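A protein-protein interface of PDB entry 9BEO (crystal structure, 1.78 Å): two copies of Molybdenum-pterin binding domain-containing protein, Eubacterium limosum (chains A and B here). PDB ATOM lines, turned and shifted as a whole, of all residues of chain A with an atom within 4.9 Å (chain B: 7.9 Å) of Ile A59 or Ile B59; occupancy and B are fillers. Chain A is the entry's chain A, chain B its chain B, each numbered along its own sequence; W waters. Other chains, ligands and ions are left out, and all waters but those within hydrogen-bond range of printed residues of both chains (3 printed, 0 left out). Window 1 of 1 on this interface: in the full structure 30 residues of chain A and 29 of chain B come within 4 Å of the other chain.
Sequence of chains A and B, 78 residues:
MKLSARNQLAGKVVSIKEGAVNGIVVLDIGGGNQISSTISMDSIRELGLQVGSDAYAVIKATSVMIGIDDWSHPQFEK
N of Ser B36 is in hydrogen-bond range of OD1 of Asn A7. The backbone carbonyl oxygen (O) of Met B65 is in hydrogen-bond range of the backbone NH (N) of Val A58 (2.8 Å). O of Val A64 is in hydrogen-bond range of OG of Ser B37, at 2.7 Å.
The backbone carbonyl oxygen (O) of Asn A7 is in hydrogen-bond range of the backbone NH (N) of Ile A59, at 2.8 Å. The backbone NH (N) of Ala A57 lies within hydrogen-bond range of the backbone carbonyl oxygen (O) of Leu A9. The backbone carbonyl oxygen of Asn B7 lies within hydrogen-bond range of the backbone NH of Ile B59 (2.9 Å).
Among the printed residues, pairs that only touch across the chains: Ile A35 with Asn B7, Asn A7 with Ile B35, Val A64 with Ser B36, Ile A59 with Ile B59, Val A64 with Val B58, Ala A57 with Met B65, Ala A61 with Ser B37, Ala A61 with Ser B36, Ser A63 with Ser B63, Val A58 with Val B64, Arg A6 with Ser B36, Ile A35 with Val B64, Val A64 with Ile B35, Val A64 with Ile B59, Leu A9 with Ile B35, Ile A59 with Val B64, Val A58 with Ser B63 and Ser A63 with Val B58.
Printed residues of chain B within 4 Å of Ile A59: Ile B59 (3.6 Å) and Val B64 (3.96 Å). Ile B59 touches two residues of chain A. Of the printed residues of chain A, Asn B7 touches Ile A35. Of the printed residues of chain A, Ile B35 touches Asn A7, Leu A9 and Val A64. Of the printed residues of chain B, Val A64 touches Ile B35 (3.9 Å), Ser B36 (3.6 Å), Ser B37 (2.7 Å), Val B58 (3.6 Å) and Ile B59 (3.9 Å). Printed residues of chain A within 4 Å of Ser B37: Ala A61 (3.6 Å) and Val A64 (2.7 Å). Printed residues of chain A within 4 Å of Val B64: Ile A35, Val A58 and Ile A59. Ala B57 touches none of the printed residues of chain A. Leu B9 touches none of the printed residues of chain A. The nearest residue of chain A that does not touch Ile B59 is Ser A63 (4.1 Å).
Among the printed residues, 21 pairs touch across the chains.
Asn A7 touches Ile B35, and with the chains exchanged Ile A35 touches Asn B7. Ile A35 touches Val B64, and with the chains exchanged Val A64 touches Ile B35. Ile A59 touches Val B64, and with the chains exchanged Val A64 touches Ile B59. Ser B63 touches its own counterpart, Ser A63. Positions printed for both chains: 5, 6, 7, 9, 35, 57, 58, 59, 60, 61, 63 and 64. Of the 21 pairs that touch across the chains among the printed residues, 12 have their exchanged pair printed and touching as well.
Water W2 bridges the side-chain hydroxyl of Ser B63 (2.6 Å) and the side-chain hydroxyl of Ser A63 (2.7 Å). Water W1 lies within hydrogen-bond range of the backbone carbonyl oxygen (O) of Ser A63, the side-chain hydroxyl (OG) of Ser B63 and the backbone NH (N) of Lys B60. Water W3 lies within hydrogen-bond range of O of Ser B63 (2.7 Å), OG of Ser A63 (2.8 Å) and N of Lys A60 (2.9 Å).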
ATOM      1  N   ALA A   5      18.093 -22.733 -30.289  1.00  0.00           N
ATOM      2  CA  ALA A   5      17.015 -22.081 -29.546  1.00  0.00           C
ATOM      3  C   ALA A   5      17.313 -20.600 -29.352  1.00  0.00           C
ATOM      4  O   ALA A   5      18.383 -20.225 -28.853  1.00  0.00           O
ATOM      5  CB  ALA A   5      16.818 -22.759 -28.186  1.00  0.00           C
ATOM      6  N   ARG A   6      16.362 -19.754 -29.761  1.00  0.00           N
ATOM      7  CA  ARG A   6      16.590 -18.314 -29.661  1.00  0.00           C
ATOM      8  C   ARG A   6      16.667 -17.850 -28.212  1.00  0.00           C
ATOM      9  O   ARG A   6      17.257 -16.789 -27.946  1.00  0.00           O
ATOM     10  CB  ARG A   6      15.464 -17.537 -30.341  1.00  0.00           C
ATOM     11  CG  ARG A   6      15.200 -17.815 -31.833  1.00  0.00           C
ATOM     12  CD  ARG A   6      16.268 -17.266 -32.738  1.00  0.00           C
ATOM     13  NE  ARG A   6      17.544 -17.948 -32.633  1.00  0.00           N
ATOM     14  CZ  ARG A   6      18.700 -17.390 -32.970  1.00  0.00           C
ATOM     15  NH1 ARG A   6      18.757 -16.157 -33.446  1.00  0.00           N
ATOM     16  NH2 ARG A   6      19.822 -18.089 -32.828  1.00  0.00           N
ATOM     17  N   ASN A   7      16.111 -18.621 -27.266  1.00  0.00           N
ATOM     18  CA  ASN A   7      16.030 -18.157 -25.884  1.00  0.00           C
ATOM     19  C   ASN A   7      16.905 -19.022 -24.992  1.00  0.00           C
ATOM     20  O   ASN A   7      16.648 -20.215 -24.838  1.00  0.00           O
ATOM     21  CB  ASN A   7      14.571 -18.151 -25.440  1.00  0.00           C
ATOM     22  CG  ASN A   7      13.710 -17.339 -26.383  1.00  0.00           C
ATOM     23  OD1 ASN A   7      13.937 -16.132 -26.552  1.00  0.00           O
ATOM     24  ND2 ASN A   7      12.728 -17.986 -27.021  1.00  0.00           N
ATOM     25  N   LEU A   9      18.414 -18.146 -21.330  1.00  0.00           N
ATOM     26  CA  LEU A   9      18.409 -17.071 -20.347  1.00  0.00           C
ATOM     27  C   LEU A   9      19.126 -17.541 -19.093  1.00  0.00           C
ATOM     28  O   LEU A   9      18.685 -18.495 -18.445  1.00  0.00           O
ATOM     29  CB  LEU A   9      16.974 -16.634 -20.039  1.00  0.00           C
ATOM     30  CG  LEU A   9      16.168 -16.310 -21.299  1.00  0.00           C
ATOM     31  CD1 LEU A   9      14.682 -16.249 -21.029  1.00  0.00           C
ATOM     32  CD2 LEU A   9      16.630 -15.000 -21.899  1.00  0.00           C
ATOM     33  N   ILE A  35      11.581 -18.209 -14.320  1.00  0.00           N
ATOM     34  CA  ILE A  35      11.099 -19.140 -15.337  1.00  0.00           C
ATOM     35  C   ILE A  35      11.021 -20.540 -14.741  1.00  0.00           C
ATOM     36  O   ILE A  35      11.983 -21.021 -14.130  1.00  0.00           O
ATOM     37  CB  ILE A  35      11.992 -19.150 -16.587  1.00  0.00           C
ATOM     38  CG1 ILE A  35      11.879 -17.796 -17.289  1.00  0.00           C
ATOM     39  CG2 ILE A  35      11.547 -20.270 -17.545  1.00  0.00           C
ATOM     40  CD1 ILE A  35      12.599 -17.727 -18.611  1.00  0.00           C
ATOM     41  N   ALA A  57      17.646 -21.084 -18.819  1.00  0.00           N
ATOM     42  CA  ALA A  57      16.331 -21.464 -19.319  1.00  0.00           C
ATOM     43  C   ALA A  57      16.385 -21.438 -20.845  1.00  0.00           C
ATOM     44  O   ALA A  57      16.614 -20.384 -21.435  1.00  0.00           O
ATOM     45  CB  ALA A  57      15.265 -20.509 -18.790  1.00  0.00           C
ATOM     46  N   VAL A  58      16.157 -22.584 -21.481  1.00  0.00           N
ATOM     47  CA  VAL A  58      16.339 -22.715 -22.924  1.00  0.00           C
ATOM     48  C   VAL A  58      14.976 -22.985 -23.539  1.00  0.00           C
ATOM     49  O   VAL A  58      14.335 -23.994 -23.220  1.00  0.00           O
ATOM     50  CB  VAL A  58      17.336 -23.828 -23.270  1.00  0.00           C
ATOM     51  CG1 VAL A  58      17.446 -23.997 -24.782  1.00  0.00           C
ATOM     52  CG2 VAL A  58      18.703 -23.523 -22.672  1.00  0.00           C
ATOM     53  N   ILE A  59      14.550 -22.091 -24.436  1.00  0.00           N
ATOM     54  CA  ILE A  59      13.202 -22.110 -24.996  1.00  0.00           C
ATOM     55  C   ILE A  59      13.298 -21.875 -26.500  1.00  0.00           C
ATOM     56  O   ILE A  59      13.865 -20.863 -26.949  1.00  0.00           O
ATOM     57  CB  ILE A  59      12.297 -21.052 -24.347  1.00  0.00           C
ATOM     58  CG1 ILE A  59      12.414 -21.142 -22.818  1.00  0.00           C
ATOM     59  CG2 ILE A  59      10.874 -21.289 -24.769  1.00  0.00           C
ATOM     60  CD1 ILE A  59      12.110 -19.876 -22.081  1.00  0.00           C
ATOM     61  N   LYS A  60      12.746 -22.814 -27.270  1.00  0.00           N
ATOM     62  CA  LYS A  60      12.673 -22.647 -28.718  1.00  0.00           C
ATOM     63  C   LYS A  60      11.675 -21.538 -29.046  1.00  0.00           C
ATOM     64  O   LYS A  60      10.647 -21.385 -28.378  1.00  0.00           O
ATOM     65  CB  LYS A  60      12.276 -23.976 -29.361  1.00  0.00           C
ATOM     66  CG  LYS A  60      12.508 -24.082 -30.862  1.00  0.00           C
ATOM     67  CD  LYS A  60      12.148 -25.462 -31.386  1.00  0.00           C
ATOM     68  CE  LYS A  60      12.515 -25.571 -32.880  1.00  0.00           C
ATOM     69  NZ  LYS A  60      11.714 -24.582 -33.652  1.00  0.00           N
ATOM     70  N   ALA A  61      11.994 -20.722 -30.055  1.00  0.00           N
ATOM     71  CA  ALA A  61      11.142 -19.570 -30.350  1.00  0.00           C
ATOM     72  C   ALA A  61       9.722 -19.978 -30.726  1.00  0.00           C
ATOM     73  O   ALA A  61       8.768 -19.252 -30.414  1.00  0.00           O
ATOM     74  CB  ALA A  61      11.752 -18.738 -31.488  1.00  0.00           C
ATOM     75  N   SER A  63       8.007 -22.115 -29.363  1.00  0.00           N
ATOM     76  CA  SER A  63       7.280 -22.473 -28.144  1.00  0.00           C
ATOM     77  C   SER A  63       6.738 -21.260 -27.392  1.00  0.00           C
ATOM     78  O   SER A  63       6.087 -21.433 -26.356  1.00  0.00           O
ATOM     79  CB  SER A  63       8.174 -23.271 -27.190  1.00  0.00           C
ATOM     80  OG  SER A  63       8.593 -24.500 -27.746  1.00  0.00           O
ATOM     81  N   VAL A  64       7.023 -20.047 -27.844  1.00  0.00           N
ATOM     82  CA  VAL A  64       6.681 -18.831 -27.113  1.00  0.00           C
ATOM     83  C   VAL A  64       5.484 -18.162 -27.762  1.00  0.00           C
ATOM     84  O   VAL A  64       5.516 -17.833 -28.959  1.00  0.00           O
ATOM     85  CB  VAL A  64       7.872 -17.858 -27.054  1.00  0.00           C
ATOM     86  CG1 VAL A  64       7.495 -16.639 -26.206  1.00  0.00           C
ATOM     87  CG2 VAL A  64       9.101 -18.544 -26.506  1.00  0.00           C
ATOM     88  N   LEU B   3      -4.324 -18.040 -17.696  1.00  0.00           N
ATOM     89  CA  LEU B   3      -3.761 -19.194 -18.389  1.00  0.00           C
ATOM     90  C   LEU B   3      -2.896 -20.039 -17.463  1.00  0.00           C
ATOM     91  O   LEU B   3      -2.215 -19.526 -16.563  1.00  0.00           O
ATOM     92  CB  LEU B   3      -2.920 -18.773 -19.628  1.00  0.00           C
ATOM     93  CG  LEU B   3      -2.588 -19.915 -20.609  1.00  0.00           C
ATOM     94  CD1 LEU B   3      -3.847 -20.377 -21.313  1.00  0.00           C
ATOM     95  CD2 LEU B   3      -1.546 -19.497 -21.656  1.00  0.00           C
ATOM     96  N   SER B   4      -2.881 -21.347 -17.740  1.00  0.00           N
ATOM     97  CA  SER B   4      -2.085 -22.261 -16.924  1.00  0.00           C
ATOM     98  C   SER B   4      -0.580 -22.094 -17.120  1.00  0.00           C
ATOM     99  O   SER B   4       0.189 -22.490 -16.234  1.00  0.00           O
ATOM    100  CB  SER B   4      -2.462 -23.704 -17.243  1.00  0.00           C
ATOM    101  OG  SER B   4      -2.047 -24.063 -18.561  1.00  0.00           O
ATOM    102  N   ALA B   5      -0.140 -21.543 -18.254  1.00  0.00           N
ATOM    103  CA  ALA B   5       1.288 -21.439 -18.539  1.00  0.00           C
ATOM    104  C   ALA B   5       2.034 -20.836 -17.357  1.00  0.00           C
ATOM    105  O   ALA B   5       1.658 -19.779 -16.850  1.00  0.00           O
ATOM    106  CB  ALA B   5       1.518 -20.576 -19.783  1.00  0.00           C
ATOM    107  N   ARG B   6       3.072 -21.538 -16.889  1.00  0.00           N
ATOM    108  CA  ARG B   6       3.770 -21.045 -15.714  1.00  0.00           C
ATOM    109  C   ARG B   6       4.528 -19.767 -16.010  1.00  0.00           C
ATOM    110  O   ARG B   6       4.760 -18.981 -15.084  1.00  0.00           O
ATOM    111  CB  ARG B   6       4.784 -22.066 -15.192  1.00  0.00           C
ATOM    112  CG  ARG B   6       4.272 -23.443 -14.854  1.00  0.00           C
ATOM    113  CD  ARG B   6       3.397 -23.480 -13.675  1.00  0.00           C
ATOM    114  NE  ARG B   6       2.122 -22.821 -13.905  1.00  0.00           N
ATOM    115  CZ  ARG B   6       1.372 -22.344 -12.923  1.00  0.00           C
ATOM    116  NH1 ARG B   6       1.743 -22.480 -11.659  1.00  0.00           N
ATOM    117  NH2 ARG B   6       0.247 -21.694 -13.219  1.00  0.00           N
ATOM    118  N   ASN B   7       4.870 -19.502 -17.271  1.00  0.00           N
ATOM    119  CA  ASN B   7       5.726 -18.359 -17.565  1.00  0.00           C
ATOM    120  C   ASN B   7       4.925 -17.336 -18.356  1.00  0.00           C
ATOM    121  O   ASN B   7       4.472 -17.624 -19.468  1.00  0.00           O
ATOM    122  CB  ASN B   7       6.968 -18.839 -18.312  1.00  0.00           C
ATOM    123  CG  ASN B   7       7.671 -19.966 -17.559  1.00  0.00           C
ATOM    124  OD1 ASN B   7       8.155 -19.768 -16.436  1.00  0.00           O
ATOM    125  ND2 ASN B   7       7.656 -21.170 -18.128  1.00  0.00           N
ATOM    126  N   GLN B   8       4.724 -16.150 -17.767  1.00  0.00           N
ATOM    127  CA  GLN B   8       3.997 -15.050 -18.411  1.00  0.00           C
ATOM    128  C   GLN B   8       4.789 -13.784 -18.073  1.00  0.00           C
ATOM    129  O   GLN B   8       4.546 -13.142 -17.049  1.00  0.00           O
ATOM    130  CB  GLN B   8       2.545 -14.979 -17.933  1.00  0.00           C
ATOM    131  CG  GLN B   8       1.793 -16.314 -18.105  1.00  0.00           C
ATOM    132  CD  GLN B   8       0.362 -16.304 -17.607  1.00  0.00           C
ATOM    133  OE1 GLN B   8      -0.259 -15.248 -17.458  1.00  0.00           O
ATOM    134  NE2 GLN B   8      -0.176 -17.504 -17.331  1.00  0.00           N
ATOM    135  N   LEU B   9       5.728 -13.419 -18.952  1.00  0.00           N
ATOM    136  CA  LEU B   9       6.761 -12.430 -18.639  1.00  0.00           C
ATOM    137  C   LEU B   9       6.464 -11.126 -19.365  1.00  0.00           C
ATOM    138  O   LEU B   9       6.471 -11.085 -20.603  1.00  0.00           O
ATOM    139  CB  LEU B   9       8.145 -12.961 -19.020  1.00  0.00           C
ATOM    140  CG  LEU B   9       8.384 -14.340 -18.413  1.00  0.00           C
ATOM    141  CD1 LEU B   9       9.533 -15.050 -19.072  1.00  0.00           C
ATOM    142  CD2 LEU B   9       8.678 -14.163 -16.937  1.00  0.00           C
ATOM    143  N   ILE B  29      12.220  -8.007 -21.724  1.00  0.00           N
ATOM    144  CA  ILE B  29      11.545  -8.350 -20.473  1.00  0.00           C
ATOM    145  C   ILE B  29      12.277  -7.795 -19.252  1.00  0.00           C
ATOM    146  O   ILE B  29      11.908  -8.116 -18.119  1.00  0.00           O
ATOM    147  CB  ILE B  29      11.324  -9.871 -20.332  1.00  0.00           C
ATOM    148  CG1 ILE B  29      12.651 -10.633 -20.306  1.00  0.00           C
ATOM    149  CG2 ILE B  29      10.387 -10.382 -21.441  1.00  0.00           C
ATOM    150  CD1 ILE B  29      12.486 -12.103 -19.859  1.00  0.00           C
ATOM    151  N   ILE B  35      13.274 -12.021 -25.169  1.00  0.00           N
ATOM    152  CA  ILE B  35      12.691 -13.301 -25.567  1.00  0.00           C
ATOM    153  C   ILE B  35      12.157 -13.179 -26.987  1.00  0.00           C
ATOM    154  O   ILE B  35      11.425 -12.233 -27.298  1.00  0.00           O
ATOM    155  CB  ILE B  35      11.579 -13.766 -24.606  1.00  0.00           C
ATOM    156  CG1 ILE B  35      12.192 -14.155 -23.259  1.00  0.00           C
ATOM    157  CG2 ILE B  35      10.831 -14.965 -25.206  1.00  0.00           C
ATOM    158  CD1 ILE B  35      11.201 -14.756 -22.296  1.00  0.00           C
ATOM    159  N   SER B  36      12.488 -14.161 -27.827  1.00  0.00           N
ATOM    160  CA  SER B  36      11.985 -14.233 -29.195  1.00  0.00           C
ATOM    161  C   SER B  36      10.830 -15.224 -29.280  1.00  0.00           C
ATOM    162  O   SER B  36      10.871 -16.306 -28.683  1.00  0.00           O
ATOM    163  CB  SER B  36      13.075 -14.662 -30.181  1.00  0.00           C
ATOM    164  OG  SER B  36      14.162 -13.751 -30.167  1.00  0.00           O
ATOM    165  N   SER B  37       9.813 -14.843 -30.032  1.00  0.00           N
ATOM    166  CA  SER B  37       8.593 -15.616 -30.201  1.00  0.00           C
ATOM    167  C   SER B  37       8.265 -15.736 -31.685  1.00  0.00           C
ATOM    168  O   SER B  37       8.064 -14.722 -32.352  1.00  0.00           O
ATOM    169  CB  SER B  37       7.450 -14.929 -29.467  1.00  0.00           C
ATOM    170  OG  SER B  37       6.199 -15.420 -29.904  1.00  0.00           O
ATOM    171  N   TYR B  56       3.306  -9.763 -23.309  1.00  0.00           N
ATOM    172  CA  TYR B  56       3.824 -10.805 -22.444  1.00  0.00           C
ATOM    173  C   TYR B  56       4.355 -11.948 -23.290  1.00  0.00           C
ATOM    174  O   TYR B  56       3.729 -12.338 -24.276  1.00  0.00           O
ATOM    175  CB  TYR B  56       2.759 -11.375 -21.509  1.00  0.00           C
ATOM    176  CG  TYR B  56       2.073 -10.391 -20.601  1.00  0.00           C
ATOM    177  CD1 TYR B  56       1.067  -9.564 -21.074  1.00  0.00           C
ATOM    178  CD2 TYR B  56       2.412 -10.314 -19.254  1.00  0.00           C
ATOM    179  CE1 TYR B  56       0.425  -8.671 -20.237  1.00  0.00           C
ATOM    180  CE2 TYR B  56       1.769  -9.429 -18.409  1.00  0.00           C
ATOM    181  CZ  TYR B  56       0.781  -8.613 -18.904  1.00  0.00           C
ATOM    182  OH  TYR B  56       0.139  -7.726 -18.063  1.00  0.00           O
ATOM    183  N   ALA B  57       5.487 -12.497 -22.874  1.00  0.00           N
ATOM    184  CA  ALA B  57       6.000 -13.750 -23.408  1.00  0.00           C
ATOM    185  C   ALA B  57       5.422 -14.886 -22.577  1.00  0.00           C
ATOM    186  O   ALA B  57       5.678 -14.969 -21.371  1.00  0.00           O
ATOM    187  CB  ALA B  57       7.527 -13.774 -23.367  1.00  0.00           C
ATOM    188  N   VAL B  58       4.673 -15.771 -23.224  1.00  0.00           N
ATOM    189  CA  VAL B  58       3.922 -16.825 -22.539  1.00  0.00           C
ATOM    190  C   VAL B  58       4.508 -18.167 -22.956  1.00  0.00           C
ATOM    191  O   VAL B  58       4.606 -18.461 -24.156  1.00  0.00           O
ATOM    192  CB  VAL B  58       2.423 -16.738 -22.855  1.00  0.00           C
ATOM    193  CG1 VAL B  58       1.682 -17.879 -22.198  1.00  0.00           C
ATOM    194  CG2 VAL B  58       1.876 -15.382 -22.384  1.00  0.00           C
ATOM    195  N   ILE B  59       4.960 -18.950 -21.971  1.00  0.00           N
ATOM    196  CA  ILE B  59       5.670 -20.205 -22.225  1.00  0.00           C
ATOM    197  C   ILE B  59       5.176 -21.259 -21.241  1.00  0.00           C
ATOM    198  O   ILE B  59       5.274 -21.070 -20.013  1.00  0.00           O
ATOM    199  CB  ILE B  59       7.196 -20.045 -22.098  1.00  0.00           C
ATOM    200  CG1 ILE B  59       7.647 -18.797 -22.868  1.00  0.00           C
ATOM    201  CG2 ILE B  59       7.908 -21.328 -22.638  1.00  0.00           C
ATOM    202  CD1 ILE B  59       8.928 -18.155 -22.364  1.00  0.00           C
ATOM    203  N   LYS B  60       4.685 -22.378 -21.780  1.00  0.00           N
ATOM    204  CA  LYS B  60       4.304 -23.527 -20.966  1.00  0.00           C
ATOM    205  C   LYS B  60       5.556 -24.143 -20.358  1.00  0.00           C
ATOM    206  O   LYS B  60       6.612 -24.208 -20.999  1.00  0.00           O
ATOM    207  CB  LYS B  60       3.581 -24.539 -21.845  1.00  0.00           C
ATOM    208  CG  LYS B  60       2.808 -25.599 -21.128  1.00  0.00           C
ATOM    209  CD  LYS B  60       2.052 -26.457 -22.145  1.00  0.00           C
ATOM    210  CE  LYS B  60       1.125 -27.432 -21.392  1.00  0.00           C
ATOM    211  NZ  LYS B  60       1.918 -28.349 -20.530  1.00  0.00           N
ATOM    212  N   ALA B  61       5.458 -24.571 -19.101  1.00  0.00           N
ATOM    213  CA  ALA B  61       6.648 -25.069 -18.423  1.00  0.00           C
ATOM    214  C   ALA B  61       7.232 -26.290 -19.118  1.00  0.00           C
ATOM    215  O   ALA B  61       8.447 -26.487 -19.098  1.00  0.00           O
ATOM    216  CB  ALA B  61       6.331 -25.395 -16.956  1.00  0.00           C
ATOM    217  N   THR B  62       6.391 -27.114 -19.756  1.00  0.00           N
ATOM    218  CA  THR B  62       6.903 -28.293 -20.435  1.00  0.00           C
ATOM    219  C   THR B  62       7.687 -27.943 -21.687  1.00  0.00           C
ATOM    220  O   THR B  62       8.264 -28.848 -22.300  1.00  0.00           O
ATOM    221  CB  THR B  62       5.762 -29.258 -20.796  1.00  0.00           C
ATOM    222  OG1 THR B  62       4.684 -28.523 -21.378  1.00  0.00           O
ATOM    223  CG2 THR B  62       5.257 -29.972 -19.542  1.00  0.00           C
ATOM    224  N   SER B  63       7.708 -26.673 -22.080  1.00  0.00           N
ATOM    225  CA  SER B  63       8.487 -26.222 -23.231  1.00  0.00           C
ATOM    226  C   SER B  63       9.872 -25.722 -22.854  1.00  0.00           C
ATOM    227  O   SER B  63      10.665 -25.417 -23.752  1.00  0.00           O
ATOM    228  CB  SER B  63       7.754 -25.094 -23.967  1.00  0.00           C
ATOM    229  OG  SER B  63       6.524 -25.539 -24.476  1.00  0.00           O
ATOM    230  N   VAL B  64      10.184 -25.628 -21.565  1.00  0.00           N
ATOM    231  CA  VAL B  64      11.427 -25.013 -21.108  1.00  0.00           C
ATOM    232  C   VAL B  64      12.400 -26.115 -20.734  1.00  0.00           C
ATOM    233  O   VAL B  64      12.086 -26.972 -19.898  1.00  0.00           O
ATOM    234  CB  VAL B  64      11.189 -24.076 -19.917  1.00  0.00           C
ATOM    235  CG1 VAL B  64      12.510 -23.376 -19.555  1.00  0.00           C
ATOM    236  CG2 VAL B  64      10.073 -23.071 -20.225  1.00  0.00           C
ATOM    237  N   MET B  65      13.576 -26.093 -21.347  1.00  0.00           N
ATOM    238  CA  MET B  65      14.687 -26.953 -20.985  1.00  0.00           C
ATOM    239  C   MET B  65      15.647 -26.190 -20.086  1.00  0.00           C
ATOM    240  O   MET B  65      15.646 -24.963 -20.051  1.00  0.00           O
ATOM    241  CB  MET B  65      15.402 -27.436 -22.247  1.00  0.00           C
ATOM    242  CG  MET B  65      14.603 -28.458 -23.007  1.00  0.00           C
ATOM    243  SD  MET B  65      15.011 -28.393 -24.760  1.00  0.00           S
ATOM    244  CE  MET B  65      14.001 -26.949 -25.129  1.00  0.00           C
ATOM    245  N   ILE B  66      16.489 -26.930 -19.365  1.00  0.00           N
ATOM    246  CA  ILE B  66      17.537 -26.328 -18.551  1.00  0.00           C
ATOM    247  C   ILE B  66      18.874 -26.701 -19.159  1.00  0.00           C
ATOM    248  O   ILE B  66      19.099 -27.866 -19.504  1.00  0.00           O
ATOM    249  CB  ILE B  66      17.487 -26.775 -17.081  1.00  0.00           C
ATOM    250  CG1 ILE B  66      16.180 -26.351 -16.398  1.00  0.00           C
ATOM    251  CG2 ILE B  66      18.672 -26.168 -16.335  1.00  0.00           C
ATOM    252  CD1 ILE B  66      15.962 -24.854 -16.312  1.00  0.00           C
HETATM  253  O   HOH W   1       4.908 -23.164 -24.660  1.00  0.00           O
HETATM  254  O   HOH W   2       6.891 -26.489 -26.907  1.00  0.00           O
HETATM  255  O   HOH W   3      10.997 -25.037 -26.445  1.00  0.00           O
